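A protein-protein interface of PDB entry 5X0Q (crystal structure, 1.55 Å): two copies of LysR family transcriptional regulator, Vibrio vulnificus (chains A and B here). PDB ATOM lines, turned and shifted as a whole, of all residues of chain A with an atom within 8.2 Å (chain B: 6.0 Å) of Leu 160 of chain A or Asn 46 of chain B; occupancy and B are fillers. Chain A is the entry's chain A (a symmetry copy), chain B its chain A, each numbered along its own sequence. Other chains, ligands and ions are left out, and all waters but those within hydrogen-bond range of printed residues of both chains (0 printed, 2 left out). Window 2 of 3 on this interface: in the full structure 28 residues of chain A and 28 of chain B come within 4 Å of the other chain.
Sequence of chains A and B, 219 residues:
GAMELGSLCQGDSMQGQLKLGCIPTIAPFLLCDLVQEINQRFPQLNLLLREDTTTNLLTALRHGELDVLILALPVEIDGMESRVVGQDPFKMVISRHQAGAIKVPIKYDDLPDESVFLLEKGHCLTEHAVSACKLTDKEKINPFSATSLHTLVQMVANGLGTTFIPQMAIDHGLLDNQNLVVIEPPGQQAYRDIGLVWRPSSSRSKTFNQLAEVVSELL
No position is printed for both chains.
Printed residues of chain B within 4 Å of Met 155 of chain A: Leu 47 (3.6 Å) and Leu 48 (3.8 Å).
Val 156 of chain A touches none of the printed residues of chain B.
Of the printed residues of chain A, Ile 38 of chain B touches Asn 158.
Asn 46 of chain B touches just these residues of chain A: Asn 158 (3.5 Å) and Leu 160 (3.5 Å).
The nearest residue of chain B that does not touch Leu 160 of chain A is Leu 45 of chain B (5.5 Å).
The nearest printed residue of chain A that does not touch Leu 45 of chain B is Leu 160 of chain A (5.5 Å).
N of Leu 47 of chain B sits at hydrogen-bond distance from OD1 of Asn 158 of chain A, 2.8 Å away.
The backbone NH (N) of Asn 46 of chain B is in hydrogen-bond range of the backbone carbonyl oxygen (O) of Gly 16 of chain B.
The backbone carbonyl oxygen (O) of Leu 18 of chain B lies within hydrogen-bond range of the backbone NH (N) of Leu 48 of chain B (2.8 Å).
O of Met 155 of chain A sits at hydrogen-bond distance from N of Leu 160 of chain A, 3.2 Å away.
The side-chain amide oxygen (OD1) of Asn 142 of chain A lies within hydrogen-bond range of the backbone NH (N) of Phe 144 of chain A.
The backbone NH (N) of Phe 117 of chain A sits at hydrogen-bond distance from the backbone carbonyl oxygen (O) of Thr 162 of chain A (3.0 Å).
The backbone carbonyl oxygen (O) of Phe 117 of chain A is in hydrogen-bond range of the side-chain hydroxyl (OG1) of Thr 163 of chain A, 2.6 Å away.
Among the printed residues, merely in contact across the chains: Leu 160 of chain A with Asn 46 of chain B, Leu 160 of chain A with Leu 47 of chain B, Asn 158 of chain A with Asn 46 of chain B, Met 155 of chain A with Leu 47 of chain B, Asn 158 of chain A with Leu 45 of chain B, Asn 158 of chain A with Ile 38 of chain B, Met 155 of chain A with Leu 48 of chain B, Phe 144 of chain A with Leu 48 of chain B, Leu 160 of chain A with Leu 48 of chain B and Phe 117 of chain A with Leu 48 of chain B.
Of the 13 printed residues of chain B, 5 touch a printed residue of chain A.
Printed residues of chain A that touch a printed residue of chain B: Phe 117, Phe 144, Met 155, Asn 158 and Leu 160.
Hydrophobic or aromatic side chains of chain A within 4 Å of the printed part of chain B: Phe 117, Phe 144, Met 155 and Leu 160.
Among the printed residues, no Asp or Glu carboxylate lies within 4 Å of a Lys or Arg side-chain nitrogen of the other chain.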
ATOM      1  N   ILE A  94      19.228  20.632  37.399  1.00  0.00           N
ATOM      2  CA  ILE A  94      18.348  21.104  36.335  1.00  0.00           C
ATOM      3  C   ILE A  94      17.989  22.550  36.642  1.00  0.00           C
ATOM      4  O   ILE A  94      17.979  22.970  37.799  1.00  0.00           O
ATOM      5  CB  ILE A  94      17.046  20.267  36.194  1.00  0.00           C
ATOM      6  CG1 ILE A  94      16.234  20.286  37.496  1.00  0.00           C
ATOM      7  CG2 ILE A  94      17.340  18.853  35.773  1.00  0.00           C
ATOM      8  CD1 ILE A  94      14.905  19.567  37.355  1.00  0.00           C
ATOM      9  N   SER A  95      17.681  23.321  35.604  1.00  0.00           N
ATOM     10  CA  SER A  95      17.232  24.683  35.871  1.00  0.00           C
ATOM     11  C   SER A  95      15.865  24.672  36.543  1.00  0.00           C
ATOM     12  O   SER A  95      15.013  23.817  36.275  1.00  0.00           O
ATOM     13  CB  SER A  95      17.144  25.489  34.578  1.00  0.00           C
ATOM     14  OG  SER A  95      16.207  24.873  33.732  1.00  0.00           O
ATOM     15  N   HIS A  97      13.515  26.542  35.853  1.00  0.00           N
ATOM     16  CA  HIS A  97      12.469  26.761  34.863  1.00  0.00           C
ATOM     17  C   HIS A  97      12.203  25.541  33.986  1.00  0.00           C
ATOM     18  O   HIS A  97      11.220  25.548  33.239  1.00  0.00           O
ATOM     19  CB  HIS A  97      12.777  28.004  34.009  1.00  0.00           C
ATOM     20  CG  HIS A  97      13.822  27.794  32.959  1.00  0.00           C
ATOM     21  ND1 HIS A  97      15.139  28.155  33.144  1.00  0.00           N
ATOM     22  CD2 HIS A  97      13.737  27.315  31.692  1.00  0.00           C
ATOM     23  CE1 HIS A  97      15.830  27.871  32.053  1.00  0.00           C
ATOM     24  NE2 HIS A  97      15.000  27.372  31.152  1.00  0.00           N
ATOM     25  N   GLN A  98      13.009  24.492  34.099  1.00  0.00           N
ATOM     26  CA  GLN A  98      12.762  23.215  33.443  1.00  0.00           C
ATOM     27  C   GLN A  98      12.408  22.139  34.453  1.00  0.00           C
ATOM     28  O   GLN A  98      12.189  20.994  34.061  1.00  0.00           O
ATOM     29  CB  GLN A  98      13.986  22.757  32.624  1.00  0.00           C
ATOM     30  CG  GLN A  98      14.379  23.656  31.432  1.00  0.00           C
ATOM     31  CD  GLN A  98      13.316  23.715  30.342  1.00  0.00           C
ATOM     32  OE1 GLN A  98      12.415  24.551  30.384  1.00  0.00           O
ATOM     33  NE2 GLN A  98      13.423  22.841  29.357  1.00  0.00           N
ATOM     34  N   ILE A 102      10.670  17.751  34.200  1.00  0.00           N
ATOM     35  CA  ILE A 102      11.422  16.551  34.556  1.00  0.00           C
ATOM     36  C   ILE A 102      10.957  16.082  35.933  1.00  0.00           C
ATOM     37  O   ILE A 102      11.022  16.842  36.906  1.00  0.00           O
ATOM     38  CB  ILE A 102      12.937  16.801  34.550  1.00  0.00           C
ATOM     39  CG1 ILE A 102      13.428  16.993  33.118  1.00  0.00           C
ATOM     40  CG2 ILE A 102      13.658  15.636  35.167  1.00  0.00           C
ATOM     41  CD1 ILE A 102      14.397  18.128  32.961  1.00  0.00           C
ATOM     42  N   PRO A 112      14.158  13.444  27.813  1.00  0.00           N
ATOM     43  CA  PRO A 112      14.276  13.542  26.356  1.00  0.00           C
ATOM     44  C   PRO A 112      15.633  13.011  25.910  1.00  0.00           C
ATOM     45  O   PRO A 112      16.619  13.056  26.653  1.00  0.00           O
ATOM     46  CB  PRO A 112      14.142  15.046  26.076  1.00  0.00           C
ATOM     47  CG  PRO A 112      13.639  15.658  27.356  1.00  0.00           C
ATOM     48  CD  PRO A 112      14.147  14.769  28.456  1.00  0.00           C
ATOM     49  N   ASP A 113      15.673  12.489  24.691  1.00  0.00           N
ATOM     50  CA  ASP A 113      16.953  12.164  24.081  1.00  0.00           C
ATOM     51  C   ASP A 113      17.826  13.416  24.043  1.00  0.00           C
ATOM     52  O   ASP A 113      17.326  14.532  23.908  1.00  0.00           O
ATOM     53  CB  ASP A 113      16.739  11.646  22.671  1.00  0.00           C
ATOM     54  CG  ASP A 113      16.282  10.195  22.634  1.00  0.00           C
ATOM     55  OD1 ASP A 113      16.121   9.700  21.506  1.00  0.00           O
ATOM     56  OD2 ASP A 113      16.133   9.534  23.681  1.00  0.00           O
ATOM     57  N   GLU A 114      19.140  13.223  24.189  1.00  0.00           N
ATOM     58  CA  GLU A 114      20.124  14.305  24.087  1.00  0.00           C
ATOM     59  C   GLU A 114      19.975  15.350  25.187  1.00  0.00           C
ATOM     60  O   GLU A 114      20.444  16.479  25.045  1.00  0.00           O
ATOM     61  CB  GLU A 114      20.058  14.966  22.703  1.00  0.00           C
ATOM     62  CG  GLU A 114      20.501  14.001  21.633  1.00  0.00           C
ATOM     63  CD  GLU A 114      20.633  14.608  20.241  1.00  0.00           C
ATOM     64  OE1 GLU A 114      20.391  15.818  20.070  1.00  0.00           O
ATOM     65  OE2 GLU A 114      20.982  13.840  19.322  1.00  0.00           O
ATOM     66  N   SER A 115      19.366  14.994  26.311  1.00  0.00           N
ATOM     67  CA  SER A 115      19.170  15.974  27.375  1.00  0.00           C
ATOM     68  C   SER A 115      20.285  15.984  28.423  1.00  0.00           C
ATOM     69  O   SER A 115      20.304  16.898  29.260  1.00  0.00           O
ATOM     70  CB  SER A 115      17.822  15.726  28.062  1.00  0.00           C
ATOM     71  OG  SER A 115      17.764  14.403  28.577  1.00  0.00           O
ATOM     72  N   VAL A 116      21.173  14.991  28.444  1.00  0.00           N
ATOM     73  CA  VAL A 116      22.249  14.911  29.438  1.00  0.00           C
ATOM     74  C   VAL A 116      23.539  15.426  28.817  1.00  0.00           C
ATOM     75  O   VAL A 116      24.079  14.816  27.886  1.00  0.00           O
ATOM     76  CB  VAL A 116      22.449  13.476  29.934  1.00  0.00           C
ATOM     77  CG1 VAL A 116      23.578  13.387  30.943  1.00  0.00           C
ATOM     78  CG2 VAL A 116      21.139  12.943  30.497  1.00  0.00           C
ATOM     79  N   PHE A 117      24.062  16.528  29.354  1.00  0.00           N
ATOM     80  CA  PHE A 117      25.312  17.101  28.896  1.00  0.00           C
ATOM     81  C   PHE A 117      26.448  16.530  29.739  1.00  0.00           C
ATOM     82  O   PHE A 117      26.314  16.362  30.968  1.00  0.00           O
ATOM     83  CB  PHE A 117      25.256  18.644  28.992  1.00  0.00           C
ATOM     84  CG  PHE A 117      24.409  19.281  27.915  1.00  0.00           C
ATOM     85  CD1 PHE A 117      23.009  19.321  28.024  1.00  0.00           C
ATOM     86  CD2 PHE A 117      25.008  19.803  26.773  1.00  0.00           C
ATOM     87  CE1 PHE A 117      22.221  19.869  27.004  1.00  0.00           C
ATOM     88  CE2 PHE A 117      24.233  20.349  25.739  1.00  0.00           C
ATOM     89  CZ  PHE A 117      22.830  20.391  25.855  1.00  0.00           C
ATOM     90  N   ASN A 142      23.687  14.344  25.159  1.00  0.00           N
ATOM     91  CA  ASN A 142      23.757  15.343  24.096  1.00  0.00           C
ATOM     92  C   ASN A 142      25.102  15.235  23.368  1.00  0.00           C
ATOM     93  O   ASN A 142      26.148  15.047  24.016  1.00  0.00           O
ATOM     94  CB  ASN A 142      23.564  16.730  24.716  1.00  0.00           C
ATOM     95  CG  ASN A 142      23.335  17.818  23.679  1.00  0.00           C
ATOM     96  OD1 ASN A 142      24.248  18.217  22.963  1.00  0.00           O
ATOM     97  ND2 ASN A 142      22.074  18.210  23.510  1.00  0.00           N
ATOM     98  N   PHE A 144      26.937  17.485  21.970  1.00  0.00           N
ATOM     99  CA  PHE A 144      27.853  18.599  22.191  1.00  0.00           C
ATOM    100  C   PHE A 144      28.488  18.412  23.560  1.00  0.00           C
ATOM    101  O   PHE A 144      27.802  18.481  24.584  1.00  0.00           O
ATOM    102  CB  PHE A 144      27.120  19.932  22.099  1.00  0.00           C
ATOM    103  CG  PHE A 144      28.028  21.113  22.285  1.00  0.00           C
ATOM    104  CD1 PHE A 144      28.202  21.650  23.541  1.00  0.00           C
ATOM    105  CD2 PHE A 144      28.721  21.640  21.209  1.00  0.00           C
ATOM    106  CE1 PHE A 144      29.063  22.751  23.745  1.00  0.00           C
ATOM    107  CE2 PHE A 144      29.584  22.726  21.395  1.00  0.00           C
ATOM    108  CZ  PHE A 144      29.752  23.263  22.659  1.00  0.00           C
ATOM    109  N   THR A 151      31.146  25.900  32.471  1.00  0.00           N
ATOM    110  CA  THR A 151      30.298  26.109  31.292  1.00  0.00           C
ATOM    111  C   THR A 151      29.299  24.977  31.134  1.00  0.00           C
ATOM    112  O   THR A 151      28.213  25.207  30.641  1.00  0.00           O
ATOM    113  CB  THR A 151      31.140  26.271  30.032  1.00  0.00           C
ATOM    114  OG1 THR A 151      32.038  25.169  29.876  1.00  0.00           O
ATOM    115  CG2 THR A 151      31.957  27.630  30.084  1.00  0.00           C
ATOM    116  N   LEU A 152      29.610  23.771  31.635  1.00  0.00           N
ATOM    117  CA  LEU A 152      28.602  22.712  31.696  1.00  0.00           C
ATOM    118  C   LEU A 152      27.400  23.174  32.525  1.00  0.00           C
ATOM    119  O   LEU A 152      26.230  23.053  32.115  1.00  0.00           O
ATOM    120  CB  LEU A 152      29.236  21.435  32.312  1.00  0.00           C
ATOM    121  CG  LEU A 152      28.340  20.238  32.617  1.00  0.00           C
ATOM    122  CD1 LEU A 152      27.574  19.821  31.371  1.00  0.00           C
ATOM    123  CD2 LEU A 152      29.137  19.047  33.211  1.00  0.00           C
ATOM    124  N   VAL A 153      27.665  23.693  33.734  1.00  0.00           N
ATOM    125  CA  VAL A 153      26.583  24.128  34.610  1.00  0.00           C
ATOM    126  C   VAL A 153      25.815  25.289  33.990  1.00  0.00           C
ATOM    127  O   VAL A 153      24.588  25.378  34.110  1.00  0.00           O
ATOM    128  CB  VAL A 153      27.146  24.529  35.984  1.00  0.00           C
ATOM    129  CG1 VAL A 153      26.080  25.215  36.832  1.00  0.00           C
ATOM    130  CG2 VAL A 153      27.698  23.302  36.727  1.00  0.00           C
ATOM    131  N   GLN A 154      26.533  26.212  33.326  1.00  0.00           N
ATOM    132  CA  GLN A 154      25.872  27.343  32.681  1.00  0.00           C
ATOM    133  C   GLN A 154      24.930  26.877  31.583  1.00  0.00           C
ATOM    134  O   GLN A 154      23.837  27.424  31.446  1.00  0.00           O
ATOM    135  CB  GLN A 154      26.915  28.308  32.115  1.00  0.00           C
ATOM    136  CG  GLN A 154      27.603  29.111  33.235  1.00  0.00           C
ATOM    137  CD  GLN A 154      29.014  29.525  32.840  1.00  0.00           C
ATOM    138  OE1 GLN A 154      29.473  29.233  31.742  1.00  0.00           O
ATOM    139  NE2 GLN A 154      29.724  30.213  33.774  1.00  0.00           N
ATOM    140  N   MET A 155      25.316  25.845  30.808  1.00  0.00           N
ATOM    141  CA  MET A 155      24.355  25.325  29.814  1.00  0.00           C
ATOM    142  C   MET A 155      23.105  24.755  30.498  1.00  0.00           C
ATOM    143  O   MET A 155      21.974  24.947  30.013  1.00  0.00           O
ATOM    144  CB  MET A 155      25.018  24.256  28.938  1.00  0.00           C
ATOM    145  CG  MET A 155      26.094  24.853  27.984  1.00  0.00           C
ATOM    146  SD  MET A 155      26.620  23.719  26.719  1.00  0.00           S
ATOM    147  CE  MET A 155      27.745  22.728  27.738  1.00  0.00           C
ATOM    148  N   VAL A 156      23.284  24.022  31.607  1.00  0.00           N
ATOM    149  CA  VAL A 156      22.117  23.546  32.358  1.00  0.00           C
ATOM    150  C   VAL A 156      21.292  24.726  32.865  1.00  0.00           C
ATOM    151  O   VAL A 156      20.063  24.740  32.739  1.00  0.00           O
ATOM    152  CB  VAL A 156      22.576  22.614  33.500  1.00  0.00           C
ATOM    153  CG1 VAL A 156      21.382  22.256  34.417  1.00  0.00           C
ATOM    154  CG2 VAL A 156      23.189  21.318  32.903  1.00  0.00           C
ATOM    155  N   ALA A 157      21.960  25.768  33.349  1.00  0.00           N
ATOM    156  CA  ALA A 157      21.250  26.937  33.850  1.00  0.00           C
ATOM    157  C   ALA A 157      20.478  27.643  32.753  1.00  0.00           C
ATOM    158  O   ALA A 157      19.458  28.293  33.029  1.00  0.00           O
ATOM    159  CB  ALA A 157      22.252  27.883  34.558  1.00  0.00           C
ATOM    160  N   ASN A 158      20.935  27.529  31.492  1.00  0.00           N
ATOM    161  CA  ASN A 158      20.250  28.076  30.336  1.00  0.00           C
ATOM    162  C   ASN A 158      19.049  27.231  29.925  1.00  0.00           C
ATOM    163  O   ASN A 158      18.292  27.636  29.044  1.00  0.00           O
ATOM    164  CB  ASN A 158      21.301  28.189  29.194  1.00  0.00           C
ATOM    165  CG  ASN A 158      20.805  28.898  27.949  1.00  0.00           C
ATOM    166  OD1 ASN A 158      21.061  28.403  26.838  1.00  0.00           O
ATOM    167  ND2 ASN A 158      20.158  30.051  28.084  1.00  0.00           N
ATOM    168  N   GLY A 159      18.805  26.108  30.619  1.00  0.00           N
ATOM    169  CA  GLY A 159      17.647  25.285  30.347  1.00  0.00           C
ATOM    170  C   GLY A 159      17.850  24.175  29.349  1.00  0.00           C
ATOM    171  O   GLY A 159      16.865  23.540  28.936  1.00  0.00           O
ATOM    172  N   LEU A 160      19.092  23.857  28.988  1.00  0.00           N
ATOM    173  CA  LEU A 160      19.294  22.963  27.855  1.00  0.00           C
ATOM    174  C   LEU A 160      19.178  21.493  28.243  1.00  0.00           C
ATOM    175  O   LEU A 160      18.996  20.646  27.365  1.00  0.00           O
ATOM    176  CB  LEU A 160      20.655  23.231  27.234  1.00  0.00           C
ATOM    177  CG  LEU A 160      20.903  24.678  26.832  1.00  0.00           C
ATOM    178  CD1 LEU A 160      22.167  24.747  25.977  1.00  0.00           C
ATOM    179  CD2 LEU A 160      19.719  25.248  26.102  1.00  0.00           C
ATOM    180  N   GLY A 161      19.271  21.162  29.525  1.00  0.00           N
ATOM    181  CA  GLY A 161      19.234  19.753  29.898  1.00  0.00           C
ATOM    182  C   GLY A 161      19.635  19.583  31.346  1.00  0.00           C
ATOM    183  O   GLY A 161      19.351  20.442  32.189  1.00  0.00           O
ATOM    184  N   THR A 162      20.293  18.458  31.624  1.00  0.00           N
ATOM    185  CA  THR A 162      20.695  18.126  32.991  1.00  0.00           C
ATOM    186  C   THR A 162      22.118  17.593  32.939  1.00  0.00           C
ATOM    187  O   THR A 162      22.690  17.389  31.863  1.00  0.00           O
ATOM    188  CB  THR A 162      19.722  17.109  33.635  1.00  0.00           C
ATOM    189  OG1 THR A 162      20.046  16.921  35.022  1.00  0.00           O
ATOM    190  CG2 THR A 162      19.806  15.751  32.906  1.00  0.00           C
ATOM    191  N   THR A 163      22.724  17.424  34.112  1.00  0.00           N
ATOM    192  CA  THR A 163      24.075  16.871  34.183  1.00  0.00           C
ATOM    193  C   THR A 163      24.350  16.426  35.600  1.00  0.00           C
ATOM    194  O   THR A 163      23.547  16.662  36.497  1.00  0.00           O
ATOM    195  CB  THR A 163      25.158  17.878  33.713  1.00  0.00           C
ATOM    196  OG1 THR A 163      26.337  17.139  33.415  1.00  0.00           O
ATOM    197  CG2 THR A 163      25.476  18.913  34.767  1.00  0.00           C
ATOM    198  N   GLN B  15      16.921  33.858  18.261  1.00  0.00           N
ATOM    199  CA  GLN B  15      16.260  32.576  18.352  1.00  0.00           C
ATOM    200  C   GLN B  15      17.236  31.489  17.944  1.00  0.00           C
ATOM    201  O   GLN B  15      18.147  31.714  17.141  1.00  0.00           O
ATOM    202  CB  GLN B  15      15.040  32.521  17.438  1.00  0.00           C
ATOM    203  CG  GLN B  15      13.899  33.401  17.867  1.00  0.00           C
ATOM    204  CD  GLN B  15      12.579  32.673  17.779  1.00  0.00           C
ATOM    205  OE1 GLN B  15      11.870  32.524  18.775  1.00  0.00           O
ATOM    206  NE2 GLN B  15      12.251  32.190  16.584  1.00  0.00           N
ATOM    207  N   GLY B  16      17.041  30.312  18.508  1.00  0.00           N
ATOM    208  CA  GLY B  16      17.767  29.152  18.060  1.00  0.00           C
ATOM    209  C   GLY B  16      19.051  28.965  18.833  1.00  0.00           C
ATOM    210  O   GLY B  16      19.198  29.434  19.962  1.00  0.00           O
ATOM    211  N   GLN B  17      19.998  28.303  18.205  1.00  0.00           N
ATOM    212  CA  GLN B  17      21.214  27.842  18.847  1.00  0.00           C
ATOM    213  C   GLN B  17      22.391  28.741  18.485  1.00  0.00           C
ATOM    214  O   GLN B  17      22.529  29.161  17.337  1.00  0.00           O
ATOM    215  CB  GLN B  17      21.479  26.418  18.397  1.00  0.00           C
ATOM    216  CG  GLN B  17      22.439  25.665  19.228  1.00  0.00           C
ATOM    217  CD  GLN B  17      22.441  24.213  18.840  1.00  0.00           C
ATOM    218  OE1 GLN B  17      21.805  23.385  19.496  1.00  0.00           O
ATOM    219  NE2 GLN B  17      23.155  23.890  17.773  1.00  0.00           N
ATOM    220  N   LEU B  18      23.241  29.035  19.464  1.00  0.00           N
ATOM    221  CA  LEU B  18      24.496  29.754  19.241  1.00  0.00           C
ATOM    222  C   LEU B  18      25.622  29.003  19.950  1.00  0.00           C
ATOM    223  O   LEU B  18      25.476  28.660  21.127  1.00  0.00           O
ATOM    224  CB  LEU B  18      24.391  31.164  19.802  1.00  0.00           C
ATOM    225  CG  LEU B  18      25.265  32.297  19.327  1.00  0.00           C
ATOM    226  CD1 LEU B  18      25.066  32.509  17.822  1.00  0.00           C
ATOM    227  CD2 LEU B  18      24.854  33.553  20.100  1.00  0.00           C
ATOM    228  N   LYS B  19      26.752  28.761  19.248  1.00  0.00           N
ATOM    229  CA  LYS B  19      27.943  28.148  19.843  1.00  0.00           C
ATOM    230  C   LYS B  19      28.897  29.269  20.216  1.00  0.00           C
ATOM    231  O   LYS B  19      29.425  29.948  19.322  1.00  0.00           O
ATOM    232  CB  LYS B  19      28.618  27.184  18.868  1.00  0.00           C
ATOM    233  CG  LYS B  19      27.732  25.930  18.582  1.00  0.00           C
ATOM    234  CD  LYS B  19      28.530  24.838  17.852  1.00  0.00           C
ATOM    235  CE  LYS B  19      27.618  23.671  17.445  1.00  0.00           C
ATOM    236  NZ  LYS B  19      28.361  22.821  16.459  1.00  0.00           N
ATOM    237  N   ILE B  38      19.876  36.275  29.436  1.00  0.00           N
ATOM    238  CA  ILE B  38      19.235  35.838  28.194  1.00  0.00           C
ATOM    239  C   ILE B  38      18.076  34.894  28.473  1.00  0.00           C
ATOM    240  O   ILE B  38      17.122  34.834  27.678  1.00  0.00           O
ATOM    241  CB  ILE B  38      20.226  35.219  27.205  1.00  0.00           C
ATOM    242  CG1 ILE B  38      20.781  33.899  27.708  1.00  0.00           C
ATOM    243  CG2 ILE B  38      21.335  36.226  26.822  1.00  0.00           C
ATOM    244  CD1 ILE B  38      21.535  33.184  26.590  1.00  0.00           C
ATOM    245  N   PHE B  42      15.740  36.718  26.154  1.00  0.00           N
ATOM    246  CA  PHE B  42      15.782  36.032  24.858  1.00  0.00           C
ATOM    247  C   PHE B  42      15.590  34.550  25.138  1.00  0.00           C
ATOM    248  O   PHE B  42      16.531  33.744  25.041  1.00  0.00           O
ATOM    249  CB  PHE B  42      17.105  36.332  24.139  1.00  0.00           C
ATOM    250  CG  PHE B  42      17.350  37.811  23.977  1.00  0.00           C
ATOM    251  CD1 PHE B  42      16.715  38.514  22.988  1.00  0.00           C
ATOM    252  CD2 PHE B  42      18.135  38.508  24.881  1.00  0.00           C
ATOM    253  CE1 PHE B  42      16.912  39.885  22.838  1.00  0.00           C
ATOM    254  CE2 PHE B  42      18.325  39.871  24.757  1.00  0.00           C
ATOM    255  CZ  PHE B  42      17.709  40.561  23.719  1.00  0.00           C
ATOM    256  N   PRO B  43      14.388  34.164  25.562  1.00  0.00           N
ATOM    257  CA  PRO B  43      14.207  32.810  26.099  1.00  0.00           C
ATOM    258  C   PRO B  43      14.302  31.723  25.049  1.00  0.00           C
ATOM    259  O   PRO B  43      14.420  30.560  25.435  1.00  0.00           O
ATOM    260  CB  PRO B  43      12.807  32.857  26.740  1.00  0.00           C
ATOM    261  CG  PRO B  43      12.143  34.001  26.151  1.00  0.00           C
ATOM    262  CD  PRO B  43      13.178  34.989  25.719  1.00  0.00           C
ATOM    263  N   GLN B  44      14.302  32.039  23.745  1.00  0.00           N
ATOM    264  CA  GLN B  44      14.471  31.001  22.736  1.00  0.00           C
ATOM    265  C   GLN B  44      15.907  30.874  22.262  1.00  0.00           C
ATOM    266  O   GLN B  44      16.174  30.145  21.303  1.00  0.00           O
ATOM    267  CB  GLN B  44      13.550  31.236  21.539  1.00  0.00           C
ATOM    268  CG  GLN B  44      12.171  30.639  21.744  1.00  0.00           C
ATOM    269  CD  GLN B  44      11.327  31.512  22.620  1.00  0.00           C
ATOM    270  OE1 GLN B  44      11.077  32.671  22.291  1.00  0.00           O
ATOM    271  NE2 GLN B  44      10.887  30.974  23.751  1.00  0.00           N
ATOM    272  N   LEU B  45      16.836  31.564  22.897  1.00  0.00           N
ATOM    273  CA  LEU B  45      18.243  31.476  22.525  1.00  0.00           C
ATOM    274  C   LEU B  45      18.923  30.403  23.379  1.00  0.00           C
ATOM    275  O   LEU B  45      18.941  30.514  24.612  1.00  0.00           O
ATOM    276  CB  LEU B  45      18.923  32.830  22.724  1.00  0.00           C
ATOM    277  CG  LEU B  45      20.402  32.894  22.318  1.00  0.00           C
ATOM    278  CD1 LEU B  45      20.538  32.503  20.892  1.00  0.00           C
ATOM    279  CD2 LEU B  45      20.969  34.289  22.510  1.00  0.00           C
ATOM    280  N   ASN B  46      19.448  29.353  22.732  1.00  0.00           N
ATOM    281  CA  ASN B  46      20.131  28.274  23.435  1.00  0.00           C
ATOM    282  C   ASN B  46      21.618  28.461  23.225  1.00  0.00           C
ATOM    283  O   ASN B  46      22.069  28.523  22.078  1.00  0.00           O
ATOM    284  CB  ASN B  46      19.712  26.900  22.928  1.00  0.00           C
ATOM    285  CG  ASN B  46      18.268  26.570  23.224  1.00  0.00           C
ATOM    286  OD1 ASN B  46      17.638  27.160  24.091  1.00  0.00           O
ATOM    287  ND2 ASN B  46      17.744  25.577  22.511  1.00  0.00           N
ATOM    288  N   LEU B  47      22.382  28.607  24.322  1.00  0.00           N
ATOM    289  CA  LEU B  47      23.803  28.889  24.236  1.00  0.00           C
ATOM    290  C   LEU B  47      24.577  27.600  24.472  1.00  0.00           C
ATOM    291  O   LEU B  47      24.661  27.145  25.611  1.00  0.00           O
ATOM    292  CB  LEU B  47      24.234  29.938  25.267  1.00  0.00           C
ATOM    293  CG  LEU B  47      24.119  31.431  24.999  1.00  0.00           C
ATOM    294  CD1 LEU B  47      24.989  32.164  26.020  1.00  0.00           C
ATOM    295  CD2 LEU B  47      24.485  31.813  23.549  1.00  0.00           C
ATOM    296  N   LEU B  48      25.206  27.049  23.427  1.00  0.00           N
ATOM    297  CA  LEU B  48      26.170  25.956  23.624  1.00  0.00           C
ATOM    298  C   LEU B  48      27.528  26.590  23.876  1.00  0.00           C
ATOM    299  O   LEU B  48      27.945  27.482  23.126  1.00  0.00           O
ATOM    300  CB  LEU B  48      26.252  25.036  22.403  1.00  0.00           C
ATOM    301  CG  LEU B  48      24.909  24.364  22.110  1.00  0.00           C
ATOM    302  CD1 LEU B  48      25.009  23.644  20.792  1.00  0.00           C
ATOM    303  CD2 LEU B  48      24.575  23.390  23.233  1.00  0.00           C
